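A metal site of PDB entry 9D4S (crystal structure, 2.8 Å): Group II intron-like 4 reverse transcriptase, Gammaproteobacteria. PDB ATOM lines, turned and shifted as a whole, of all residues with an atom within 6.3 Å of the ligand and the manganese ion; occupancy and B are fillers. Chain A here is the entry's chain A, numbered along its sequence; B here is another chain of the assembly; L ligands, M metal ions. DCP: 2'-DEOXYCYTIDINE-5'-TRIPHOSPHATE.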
ATOM      1  N   LYS A  71      14.665 -13.928   6.840  1.00  0.00           N
ATOM      2  CA  LYS A  71      13.475 -13.364   6.159  1.00  0.00           C
ATOM      3  C   LYS A  71      13.066 -12.137   6.979  1.00  0.00           C
ATOM      4  O   LYS A  71      13.468 -12.044   8.142  1.00  0.00           O
ATOM      5  CB  LYS A  71      12.334 -14.382   6.094  1.00  0.00           C
ATOM      6  CG  LYS A  71      12.206 -15.165   4.803  1.00  0.00           C
ATOM      7  CD  LYS A  71      11.078 -16.150   4.885  1.00  0.00           C
ATOM      8  CE  LYS A  71       9.820 -15.567   5.485  1.00  0.00           C
ATOM      9  NZ  LYS A  71       8.716 -16.561   5.540  1.00  0.00           N
ATOM     10  N   LYS A  75      10.963 -14.574  11.003  1.00  0.00           N
ATOM     11  CA  LYS A  75      10.694 -15.810  10.233  1.00  0.00           C
ATOM     12  C   LYS A  75      11.912 -16.234   9.408  1.00  0.00           C
ATOM     13  O   LYS A  75      12.734 -15.368   9.100  1.00  0.00           O
ATOM     14  CB  LYS A  75       9.479 -15.530   9.343  1.00  0.00           C
ATOM     15  CG  LYS A  75       8.322 -14.811  10.024  1.00  0.00           C
ATOM     16  CD  LYS A  75       7.217 -14.429   9.068  1.00  0.00           C
ATOM     17  CE  LYS A  75       6.051 -13.763   9.760  1.00  0.00           C
ATOM     18  NZ  LYS A  75       4.991 -13.375   8.813  1.00  0.00           N
ATOM     19  N   ARG A  77      13.054 -18.768   5.923  1.00  0.00           N
ATOM     20  CA  ARG A  77      12.600 -19.628   4.831  1.00  0.00           C
ATOM     21  C   ARG A  77      13.391 -20.940   4.938  1.00  0.00           C
ATOM     22  O   ARG A  77      14.621 -20.905   4.856  1.00  0.00           O
ATOM     23  CB  ARG A  77      12.793 -18.962   3.460  1.00  0.00           C
ATOM     24  CG  ARG A  77      11.931 -19.574   2.331  1.00  0.00           C
ATOM     25  CD  ARG A  77      11.620 -18.661   1.076  1.00  0.00           C
ATOM     26  NE  ARG A  77      10.829 -17.441   1.323  1.00  0.00           N
ATOM     27  CZ  ARG A  77       9.631 -17.379   1.912  1.00  0.00           C
ATOM     28  NH1 ARG A  77       8.982 -18.475   2.298  1.00  0.00           N
ATOM     29  NH2 ARG A  77       9.073 -16.188   2.138  1.00  0.00           N
ATOM     30  N   ASP A 144      -4.101 -14.769   4.781  1.00  0.00           N
ATOM     31  CA  ASP A 144      -2.955 -15.607   4.320  1.00  0.00           C
ATOM     32  C   ASP A 144      -2.825 -16.786   5.298  1.00  0.00           C
ATOM     33  O   ASP A 144      -3.293 -16.647   6.418  1.00  0.00           O
ATOM     34  CB  ASP A 144      -1.677 -14.757   4.268  1.00  0.00           C
ATOM     35  CG  ASP A 144      -0.417 -15.447   3.803  1.00  0.00           C
ATOM     36  OD1 ASP A 144       0.111 -16.274   4.556  1.00  0.00           O
ATOM     37  OD2 ASP A 144       0.057 -15.121   2.707  1.00  0.00           O
ATOM     38  N   ILE A 145      -2.196 -17.876   4.863  1.00  0.00           N
ATOM     39  CA  ILE A 145      -1.957 -19.030   5.770  1.00  0.00           C
ATOM     40  C   ILE A 145      -0.547 -18.908   6.332  1.00  0.00           C
ATOM     41  O   ILE A 145       0.397 -18.753   5.547  1.00  0.00           O
ATOM     42  CB  ILE A 145      -2.099 -20.351   4.982  1.00  0.00           C
ATOM     43  CG1 ILE A 145      -3.481 -20.486   4.338  1.00  0.00           C
ATOM     44  CG2 ILE A 145      -1.775 -21.541   5.867  1.00  0.00           C
ATOM     45  CD1 ILE A 145      -3.630 -21.737   3.506  1.00  0.00           C
ATOM     46  N   PRO A 146      -0.367 -18.926   7.667  1.00  0.00           N
ATOM     47  CA  PRO A 146       0.962 -18.908   8.257  1.00  0.00           C
ATOM     48  C   PRO A 146       1.787 -20.176   7.992  1.00  0.00           C
ATOM     49  O   PRO A 146       1.245 -21.235   8.180  1.00  0.00           O
ATOM     50  CB  PRO A 146       0.660 -18.911   9.753  1.00  0.00           C
ATOM     51  CG  PRO A 146      -0.730 -18.362   9.901  1.00  0.00           C
ATOM     52  CD  PRO A 146      -1.433 -18.864   8.665  1.00  0.00           C
ATOM     53  N   ALA A 147       3.049 -20.034   7.588  1.00  0.00           N
ATOM     54  CA  ALA A 147       3.943 -21.210   7.443  1.00  0.00           C
ATOM     55  C   ALA A 147       3.261 -22.272   6.584  1.00  0.00           C
ATOM     56  O   ALA A 147       3.312 -23.437   6.978  1.00  0.00           O
ATOM     57  CB  ALA A 147       4.328 -21.721   8.793  1.00  0.00           C
ATOM     58  N   PHE A 148       2.685 -21.898   5.451  1.00  0.00           N
ATOM     59  CA  PHE A 148       1.847 -22.873   4.711  1.00  0.00           C
ATOM     60  C   PHE A 148       2.625 -24.118   4.259  1.00  0.00           C
ATOM     61  O   PHE A 148       2.121 -25.211   4.509  1.00  0.00           O
ATOM     62  CB  PHE A 148       1.218 -22.124   3.541  1.00  0.00           C
ATOM     63  CG  PHE A 148       0.400 -22.927   2.569  1.00  0.00           C
ATOM     64  CD1 PHE A 148      -0.449 -23.932   3.008  1.00  0.00           C
ATOM     65  CD2 PHE A 148       0.436 -22.632   1.219  1.00  0.00           C
ATOM     66  CE1 PHE A 148      -1.201 -24.662   2.108  1.00  0.00           C
ATOM     67  CE2 PHE A 148      -0.328 -23.350   0.319  1.00  0.00           C
ATOM     68  CZ  PHE A 148      -1.138 -24.374   0.768  1.00  0.00           C
ATOM     69  N   PHE A 149       3.825 -23.965   3.716  1.00  0.00           N
ATOM     70  CA  PHE A 149       4.576 -25.136   3.194  1.00  0.00           C
ATOM     71  C   PHE A 149       4.938 -26.071   4.341  1.00  0.00           C
ATOM     72  O   PHE A 149       4.925 -27.283   4.159  1.00  0.00           O
ATOM     73  CB  PHE A 149       5.707 -24.687   2.258  1.00  0.00           C
ATOM     74  CG  PHE A 149       5.253 -24.412   0.843  1.00  0.00           C
ATOM     75  CD1 PHE A 149       3.962 -23.980   0.575  1.00  0.00           C
ATOM     76  CD2 PHE A 149       6.123 -24.593  -0.220  1.00  0.00           C
ATOM     77  CE1 PHE A 149       3.552 -23.725  -0.723  1.00  0.00           C
ATOM     78  CE2 PHE A 149       5.700 -24.335  -1.523  1.00  0.00           C
ATOM     79  CZ  PHE A 149       4.420 -23.908  -1.762  1.00  0.00           C
ATOM     80  N   THR A 150       5.298 -25.499   5.485  1.00  0.00           N
ATOM     81  CA  THR A 150       5.676 -26.264   6.695  1.00  0.00           C
ATOM     82  C   THR A 150       4.517 -27.128   7.203  1.00  0.00           C
ATOM     83  O   THR A 150       4.792 -28.195   7.762  1.00  0.00           O
ATOM     84  CB  THR A 150       6.139 -25.317   7.795  1.00  0.00           C
ATOM     85  OG1 THR A 150       4.981 -24.796   8.440  1.00  0.00           O
ATOM     86  CG2 THR A 150       7.003 -24.186   7.273  1.00  0.00           C
ATOM     87  N   GLN A 206      10.868 -26.478   0.470  1.00  0.00           N
ATOM     88  CA  GLN A 206      10.879 -25.188  -0.238  1.00  0.00           C
ATOM     89  C   GLN A 206      12.120 -25.266  -1.112  1.00  0.00           C
ATOM     90  O   GLN A 206      13.185 -25.523  -0.548  1.00  0.00           O
ATOM     91  CB  GLN A 206      10.783 -24.047   0.764  1.00  0.00           C
ATOM     92  CG  GLN A 206       9.352 -23.862   1.267  1.00  0.00           C
ATOM     93  CD  GLN A 206       9.185 -22.899   2.409  1.00  0.00           C
ATOM     94  OE1 GLN A 206       9.478 -21.710   2.306  1.00  0.00           O
ATOM     95  NE2 GLN A 206       8.684 -23.407   3.525  1.00  0.00           N
ATOM     96  N   GLY A 207      12.024 -24.918  -2.386  1.00  0.00           N
ATOM     97  CA  GLY A 207      13.118 -25.188  -3.341  1.00  0.00           C
ATOM     98  C   GLY A 207      12.831 -26.427  -4.166  1.00  0.00           C
ATOM     99  O   GLY A 207      13.688 -26.790  -4.982  1.00  0.00           O
ATOM    100  N   PRO A 212       4.902 -26.150  -5.061  1.00  0.00           N
ATOM    101  CA  PRO A 212       3.808 -25.226  -5.362  1.00  0.00           C
ATOM    102  C   PRO A 212       2.546 -25.935  -5.902  1.00  0.00           C
ATOM    103  O   PRO A 212       1.481 -25.553  -5.486  1.00  0.00           O
ATOM    104  CB  PRO A 212       4.447 -24.322  -6.417  1.00  0.00           C
ATOM    105  CG  PRO A 212       5.890 -24.302  -6.023  1.00  0.00           C
ATOM    106  CD  PRO A 212       6.157 -25.752  -5.701  1.00  0.00           C
ATOM    107  N   ILE A 237      -1.633 -19.039  -4.379  1.00  0.00           N
ATOM    108  CA  ILE A 237      -0.902 -19.789  -3.317  1.00  0.00           C
ATOM    109  C   ILE A 237      -1.751 -19.696  -2.053  1.00  0.00           C
ATOM    110  O   ILE A 237      -2.897 -20.099  -2.116  1.00  0.00           O
ATOM    111  CB  ILE A 237       0.560 -19.308  -3.141  1.00  0.00           C
ATOM    112  CG1 ILE A 237       1.214 -18.967  -4.481  1.00  0.00           C
ATOM    113  CG2 ILE A 237       1.381 -20.329  -2.381  1.00  0.00           C
ATOM    114  CD1 ILE A 237       1.850 -20.153  -5.156  1.00  0.00           C
ATOM    115  N   ASP A 238      -1.160 -19.349  -0.904  1.00  0.00           N
ATOM    116  CA  ASP A 238      -1.886 -19.130   0.375  1.00  0.00           C
ATOM    117  C   ASP A 238      -2.812 -17.905   0.390  1.00  0.00           C
ATOM    118  O   ASP A 238      -3.845 -17.987   1.046  1.00  0.00           O
ATOM    119  CB  ASP A 238      -0.924 -19.182   1.567  1.00  0.00           C
ATOM    120  CG  ASP A 238       0.156 -18.136   1.625  1.00  0.00           C
ATOM    121  OD1 ASP A 238       0.282 -17.361   0.665  1.00  0.00           O
ATOM    122  OD2 ASP A 238       0.852 -18.110   2.647  1.00  0.00           O
ATOM    123  N   ASP A 239      -2.423 -16.793  -0.241  1.00  0.00           N
ATOM    124  CA  ASP A 239      -3.232 -15.542  -0.091  1.00  0.00           C
ATOM    125  C   ASP A 239      -4.632 -15.730  -0.659  1.00  0.00           C
ATOM    126  O   ASP A 239      -4.757 -16.202  -1.789  1.00  0.00           O
ATOM    127  CB  ASP A 239      -2.565 -14.360  -0.781  1.00  0.00           C
ATOM    128  CG  ASP A 239      -1.384 -13.771  -0.040  1.00  0.00           C
ATOM    129  OD1 ASP A 239      -0.377 -14.484   0.110  1.00  0.00           O
ATOM    130  OD2 ASP A 239      -1.482 -12.609   0.384  1.00  0.00           O
ATOM    131  N   TYR A 269      -4.358 -15.742   9.042  1.00  0.00           N
ATOM    132  CA  TYR A 269      -4.126 -14.536   9.849  1.00  0.00           C
ATOM    133  C   TYR A 269      -5.464 -13.837  10.095  1.00  0.00           C
ATOM    134  O   TYR A 269      -6.288 -13.788   9.172  1.00  0.00           O
ATOM    135  CB  TYR A 269      -3.108 -13.664   9.125  1.00  0.00           C
ATOM    136  CG  TYR A 269      -1.687 -14.152   9.218  1.00  0.00           C
ATOM    137  CD1 TYR A 269      -0.958 -13.954  10.383  1.00  0.00           C
ATOM    138  CD2 TYR A 269      -1.081 -14.829   8.177  1.00  0.00           C
ATOM    139  CE1 TYR A 269       0.344 -14.392  10.495  1.00  0.00           C
ATOM    140  CE2 TYR A 269       0.227 -15.270   8.274  1.00  0.00           C
ATOM    141  CZ  TYR A 269       0.942 -15.060   9.438  1.00  0.00           C
ATOM    142  OH  TYR A 269       2.230 -15.489   9.575  1.00  0.00           O
ATOM    143  N   LYS A 277      -1.085  -8.931   7.429  1.00  0.00           N
ATOM    144  CA  LYS A 277      -1.361 -10.167   6.638  1.00  0.00           C
ATOM    145  C   LYS A 277      -2.846 -10.385   6.337  1.00  0.00           C
ATOM    146  O   LYS A 277      -3.138 -11.307   5.556  1.00  0.00           O
ATOM    147  CB  LYS A 277      -0.686 -11.362   7.328  1.00  0.00           C
ATOM    148  CG  LYS A 277       0.802 -11.208   7.579  1.00  0.00           C
ATOM    149  CD  LYS A 277       1.633 -12.328   7.002  1.00  0.00           C
ATOM    150  CE  LYS A 277       1.438 -12.504   5.503  1.00  0.00           C
ATOM    151  NZ  LYS A 277       2.424 -13.449   4.931  1.00  0.00           N
ATOM    152  P    DG B   3      20.000 -20.230  -5.721  1.00  0.00           P
ATOM    153  OP1  DG B   3      20.868 -20.609  -6.882  1.00  0.00           O
ATOM    154  OP2  DG B   3      19.455 -18.823  -5.785  1.00  0.00           O
ATOM    155  O5'  DG B   3      18.743 -21.203  -5.759  1.00  0.00           O
ATOM    156  C5'  DG B   3      18.971 -22.603  -5.465  1.00  0.00           C
ATOM    157  C4'  DG B   3      17.660 -23.232  -5.065  1.00  0.00           C
ATOM    158  O4'  DG B   3      17.234 -22.699  -3.792  1.00  0.00           O
ATOM    159  C3'  DG B   3      16.502 -22.940  -5.999  1.00  0.00           C
ATOM    160  O3'  DG B   3      16.505 -23.801  -7.134  1.00  0.00           O
ATOM    161  C2'  DG B   3      15.325 -23.236  -5.091  1.00  0.00           C
ATOM    162  C1'  DG B   3      15.804 -22.686  -3.767  1.00  0.00           C
ATOM    163  N9   DG B   3      15.351 -21.323  -3.527  1.00  0.00           N
ATOM    164  C8   DG B   3      16.063 -20.148  -3.540  1.00  0.00           C
ATOM    165  N7   DG B   3      15.331 -19.102  -3.270  1.00  0.00           N
ATOM    166  C5   DG B   3      14.058 -19.623  -3.048  1.00  0.00           C
ATOM    167  C6   DG B   3      12.855 -18.966  -2.712  1.00  0.00           C
ATOM    168  O6   DG B   3      12.662 -17.755  -2.539  1.00  0.00           O
ATOM    169  N1   DG B   3      11.797 -19.876  -2.582  1.00  0.00           N
ATOM    170  C2   DG B   3      11.895 -21.240  -2.763  1.00  0.00           C
ATOM    171  N2   DG B   3      10.780 -21.948  -2.605  1.00  0.00           N
ATOM    172  N3   DG B   3      13.036 -21.854  -3.071  1.00  0.00           N
ATOM    173  C4   DG B   3      14.063 -20.994  -3.191  1.00  0.00           C
ATOM    174  P    DC B   4      15.614 -23.462  -8.417  1.00  0.00           P
ATOM    175  OP1  DC B   4      15.837 -24.509  -9.471  1.00  0.00           O
ATOM    176  OP2  DC B   4      15.831 -22.060  -8.883  1.00  0.00           O
ATOM    177  O5'  DC B   4      14.090 -23.582  -7.958  1.00  0.00           O
ATOM    178  C5'  DC B   4      13.545 -24.880  -7.645  1.00  0.00           C
ATOM    179  C4'  DC B   4      12.097 -24.741  -7.246  1.00  0.00           C
ATOM    180  O4'  DC B   4      11.958 -23.874  -6.097  1.00  0.00           O
ATOM    181  C3'  DC B   4      11.233 -24.065  -8.292  1.00  0.00           C
ATOM    182  O3'  DC B   4      10.895 -24.962  -9.345  1.00  0.00           O
ATOM    183  C2'  DC B   4      10.044 -23.652  -7.448  1.00  0.00           C
ATOM    184  C1'  DC B   4      10.733 -23.182  -6.175  1.00  0.00           C
ATOM    185  N1   DC B   4      11.035 -21.737  -6.163  1.00  0.00           N
ATOM    186  C2   DC B   4      10.023 -20.856  -5.787  1.00  0.00           C
ATOM    187  O2   DC B   4       8.905 -21.304  -5.518  1.00  0.00           O
ATOM    188  N3   DC B   4      10.288 -19.535  -5.753  1.00  0.00           N
ATOM    189  C4   DC B   4      11.509 -19.078  -6.062  1.00  0.00           C
ATOM    190  N4   DC B   4      11.709 -17.768  -6.006  1.00  0.00           N
ATOM    191  C5   DC B   4      12.560 -19.960  -6.419  1.00  0.00           C
ATOM    192  C6   DC B   4      12.273 -21.270  -6.449  1.00  0.00           C
ATOM    193  P    DC B  17       5.684  -7.459  -5.479  1.00  0.00           P
ATOM    194  OP1  DC B  17       4.933  -6.481  -4.648  1.00  0.00           O
ATOM    195  OP2  DC B  17       7.060  -7.850  -5.103  1.00  0.00           O
ATOM    196  O5'  DC B  17       4.846  -8.804  -5.628  1.00  0.00           O
ATOM    197  C5'  DC B  17       3.566  -8.753  -6.139  1.00  0.00           C
ATOM    198  C4'  DC B  17       3.004 -10.131  -6.282  1.00  0.00           C
ATOM    199  O4'  DC B  17       3.647 -10.829  -7.350  1.00  0.00           O
ATOM    200  C3'  DC B  17       3.230 -11.026  -5.077  1.00  0.00           C
ATOM    201  O3'  DC B  17       2.250 -10.727  -4.120  1.00  0.00           O
ATOM    202  C2'  DC B  17       3.008 -12.407  -5.691  1.00  0.00           C
ATOM    203  C1'  DC B  17       3.581 -12.222  -7.094  1.00  0.00           C
ATOM    204  N1   DC B  17       4.926 -12.794  -7.260  1.00  0.00           N
ATOM    205  C2   DC B  17       5.048 -14.133  -7.634  1.00  0.00           C
ATOM    206  O2   DC B  17       4.030 -14.782  -7.878  1.00  0.00           O
ATOM    207  N3   DC B  17       6.306 -14.646  -7.777  1.00  0.00           N
ATOM    208  C4   DC B  17       7.370 -13.880  -7.561  1.00  0.00           C
ATOM    209  N4   DC B  17       8.566 -14.425  -7.707  1.00  0.00           N
ATOM    210  C5   DC B  17       7.255 -12.507  -7.146  1.00  0.00           C
ATOM    211  C6   DC B  17       6.033 -12.016  -7.006  1.00  0.00           C
ATOM    212  P   DDG B  18       2.410 -10.902  -2.581  1.00  0.00           P
ATOM    213  OP1 DDG B  18       1.808 -10.018  -1.585  1.00  0.00           O
ATOM    214  OP2 DDG B  18       3.927 -11.074  -2.341  1.00  0.00           O
ATOM    215  O5' DDG B  18       1.618 -12.341  -2.520  1.00  0.00           O
ATOM    216  C5' DDG B  18       2.333 -13.443  -1.980  1.00  0.00           C
ATOM    217  C4' DDG B  18       1.784 -14.743  -2.600  1.00  0.00           C
ATOM    218  O4' DDG B  18       2.544 -15.137  -3.894  1.00  0.00           O
ATOM    219  C3' DDG B  18       2.017 -15.676  -1.763  1.00  0.00           C
ATOM    220  C2' DDG B  18       3.488 -16.172  -2.115  1.00  0.00           C
ATOM    221  C1' DDG B  18       3.559 -16.129  -3.424  1.00  0.00           C
ATOM    222  N9  DDG B  18       4.918 -15.592  -3.823  1.00  0.00           N
ATOM    223  C8  DDG B  18       5.459 -14.347  -3.832  1.00  0.00           C
ATOM    224  N7  DDG B  18       6.711 -14.468  -4.294  1.00  0.00           N
ATOM    225  C5  DDG B  18       6.906 -15.762  -4.564  1.00  0.00           C
ATOM    226  C6  DDG B  18       8.121 -16.536  -5.105  1.00  0.00           C
ATOM    227  O6  DDG B  18       9.156 -15.931  -5.384  1.00  0.00           O
ATOM    228  N1  DDG B  18       8.004 -17.944  -5.277  1.00  0.00           N
ATOM    229  C2  DDG B  18       6.797 -18.649  -4.954  1.00  0.00           C
ATOM    230  N2  DDG B  18       6.727 -20.050  -5.142  1.00  0.00           N
ATOM    231  N3  DDG B  18       5.666 -17.929  -4.444  1.00  0.00           N
ATOM    232  C4  DDG B  18       5.777 -16.451  -4.254  1.00  0.00           C
HETATM  233  N1  DCP L   1       7.044 -19.354  -1.268  1.00  0.00           N
HETATM  234  C2  DCP L   1       8.266 -19.815  -1.797  1.00  0.00           C
HETATM  235  N3  DCP L   1       9.223 -18.921  -2.100  1.00  0.00           N
HETATM  236  C4  DCP L   1       9.018 -17.604  -1.911  1.00  0.00           C
HETATM  237  C5  DCP L   1       7.777 -17.105  -1.389  1.00  0.00           C
HETATM  238  C6  DCP L   1       6.846 -18.005  -1.076  1.00  0.00           C
HETATM  239  O2  DCP L   1       8.422 -21.023  -1.953  1.00  0.00           O
HETATM  240  N4  DCP L   1      10.007 -16.769  -2.212  1.00  0.00           N
HETATM  241  C1' DCP L   1       6.013 -20.361  -0.922  1.00  0.00           C
HETATM  242  C2' DCP L   1       6.331 -21.157   0.347  1.00  0.00           C
HETATM  243  C3' DCP L   1       5.539 -20.416   1.407  1.00  0.00           C
HETATM  244  C4' DCP L   1       4.285 -20.058   0.626  1.00  0.00           C
HETATM  245  O4' DCP L   1       4.786 -19.687  -0.677  1.00  0.00           O
HETATM  246  O3' DCP L   1       5.268 -21.228   2.546  1.00  0.00           O
HETATM  247  C5' DCP L   1       3.420 -18.966   1.215  1.00  0.00           C
HETATM  248  O5' DCP L   1       4.090 -17.702   1.062  1.00  0.00           O
HETATM  249  PA  DCP L   1       4.194 -16.675   2.242  1.00  0.00           P
HETATM  250  O1A DCP L   1       5.090 -15.576   1.860  1.00  0.00           O
HETATM  251  O2A DCP L   1       2.778 -16.263   2.682  1.00  0.00           O
HETATM  252  O3A DCP L   1       4.937 -17.489   3.399  1.00  0.00           O
HETATM  253  PB  DCP L   1       4.552 -18.371   4.672  1.00  0.00           P
HETATM  254  O1B DCP L   1       5.533 -19.461   4.783  1.00  0.00           O
HETATM  255  O2B DCP L   1       3.088 -18.803   4.574  1.00  0.00           O
HETATM  256  O3B DCP L   1       4.701 -17.313   5.814  1.00  0.00           O
HETATM  257  PG  DCP L   1       3.831 -16.284   6.664  1.00  0.00           P
HETATM  258  O1G DCP L   1       3.514 -16.873   7.961  1.00  0.00           O
HETATM  259  O2G DCP L   1       4.709 -15.050   6.783  1.00  0.00           O
HETATM  260  O3G DCP L   1       2.609 -15.968   5.772  1.00  0.00           O
HETATM  261 MN    MN M   1       1.618 -17.350   4.429  1.00  0.00          MN
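An oxygen (O1G) of the ligand sits at hydrogen-bond distance from the side-chain hydroxyl of Tyr 269. O6 of DG 3 of chain B is in hydrogen-bond range of N4 of the ligand. The side-chain amino group (NZ) of Lys 75 lies within salt-bridge range of an oxygen (O2G) of the ligand (2.6 Å). NZ of Lys 277 lies within salt-bridge range of O2G of the ligand. N of Ala 147 lies within hydrogen-bond range of O1G of the ligand (3.2 Å). N of Phe 148 sits close to O2B of the ligand (3.2 Å). N of Phe 149 sits at hydrogen-bond distance from O3' of the ligand (3.3 Å). O6 of DDG 18 of chain B is in hydrogen-bond range of N4 of the ligand (3.4 Å).
The backbone NH (N) of Tyr 269 sits at hydrogen-bond distance from the backbone carbonyl oxygen (O) of Asp 144, at 3.0 Å. OD2 of Asp 144 is in salt-bridge range of NZ of Lys 277, at 3.7 Å. The side-chain carboxylate (OD1) of Asp 239 lies close to the side-chain carboxylate (OD2) of Asp 144 (2.7 Å). N2 of DG 3 of chain B is in hydrogen-bond range of the backbone NH of Gly 207 (3.2 Å). OG1 of Thr 150 sits at hydrogen-bond distance from O of Ala 147, 2.6 Å away. N2 of DDG 18 of chain B lies close to O2 of DC 4 of chain B (2.5 Å). The guanidinium group of Arg 77 lies close to the side-chain amide oxygen of Gln 206 (3.3 Å).
Merely in contact with the ligand: Pro 146 (3.3 Å), DC 4 of chain B (3.6 Å), Arg 77 (3.7 Å), Gln 206 (3.7 Å) and Ile 237 (3.9 Å). Hydrophobic or aromatic side chains that line the ligand: Pro 146, Phe 148, Phe 149, Ile 237 and Tyr 269. Of the 22 residues printed, 16 come within 4 Å of the ligand. The nearest printed residue that does not touch the ligand is Lys 71 (4.1 Å).
Three residues have an atom within 4 Å of the manganese ion: Asp 144, Ile 145 and Asp 238. The nearest printed residue that does not touch the manganese ion is Lys 277 (4.01 Å).
OD1 of Asp 144 binds the manganese ion. O2B of the ligand is bound to the manganese ion (2.1 Å). The side-chain carboxylate (OD2) of Asp 238 binds the manganese ion, 2.1 Å away. O3G of the ligand is bound to the manganese ion. The backbone carbonyl oxygen (O) of Ile 145 binds the manganese ion (2.2 Å). The manganese ion is bound by O2A of the ligand (2.4 Å). The manganese ion has six donor atoms within binding distance.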
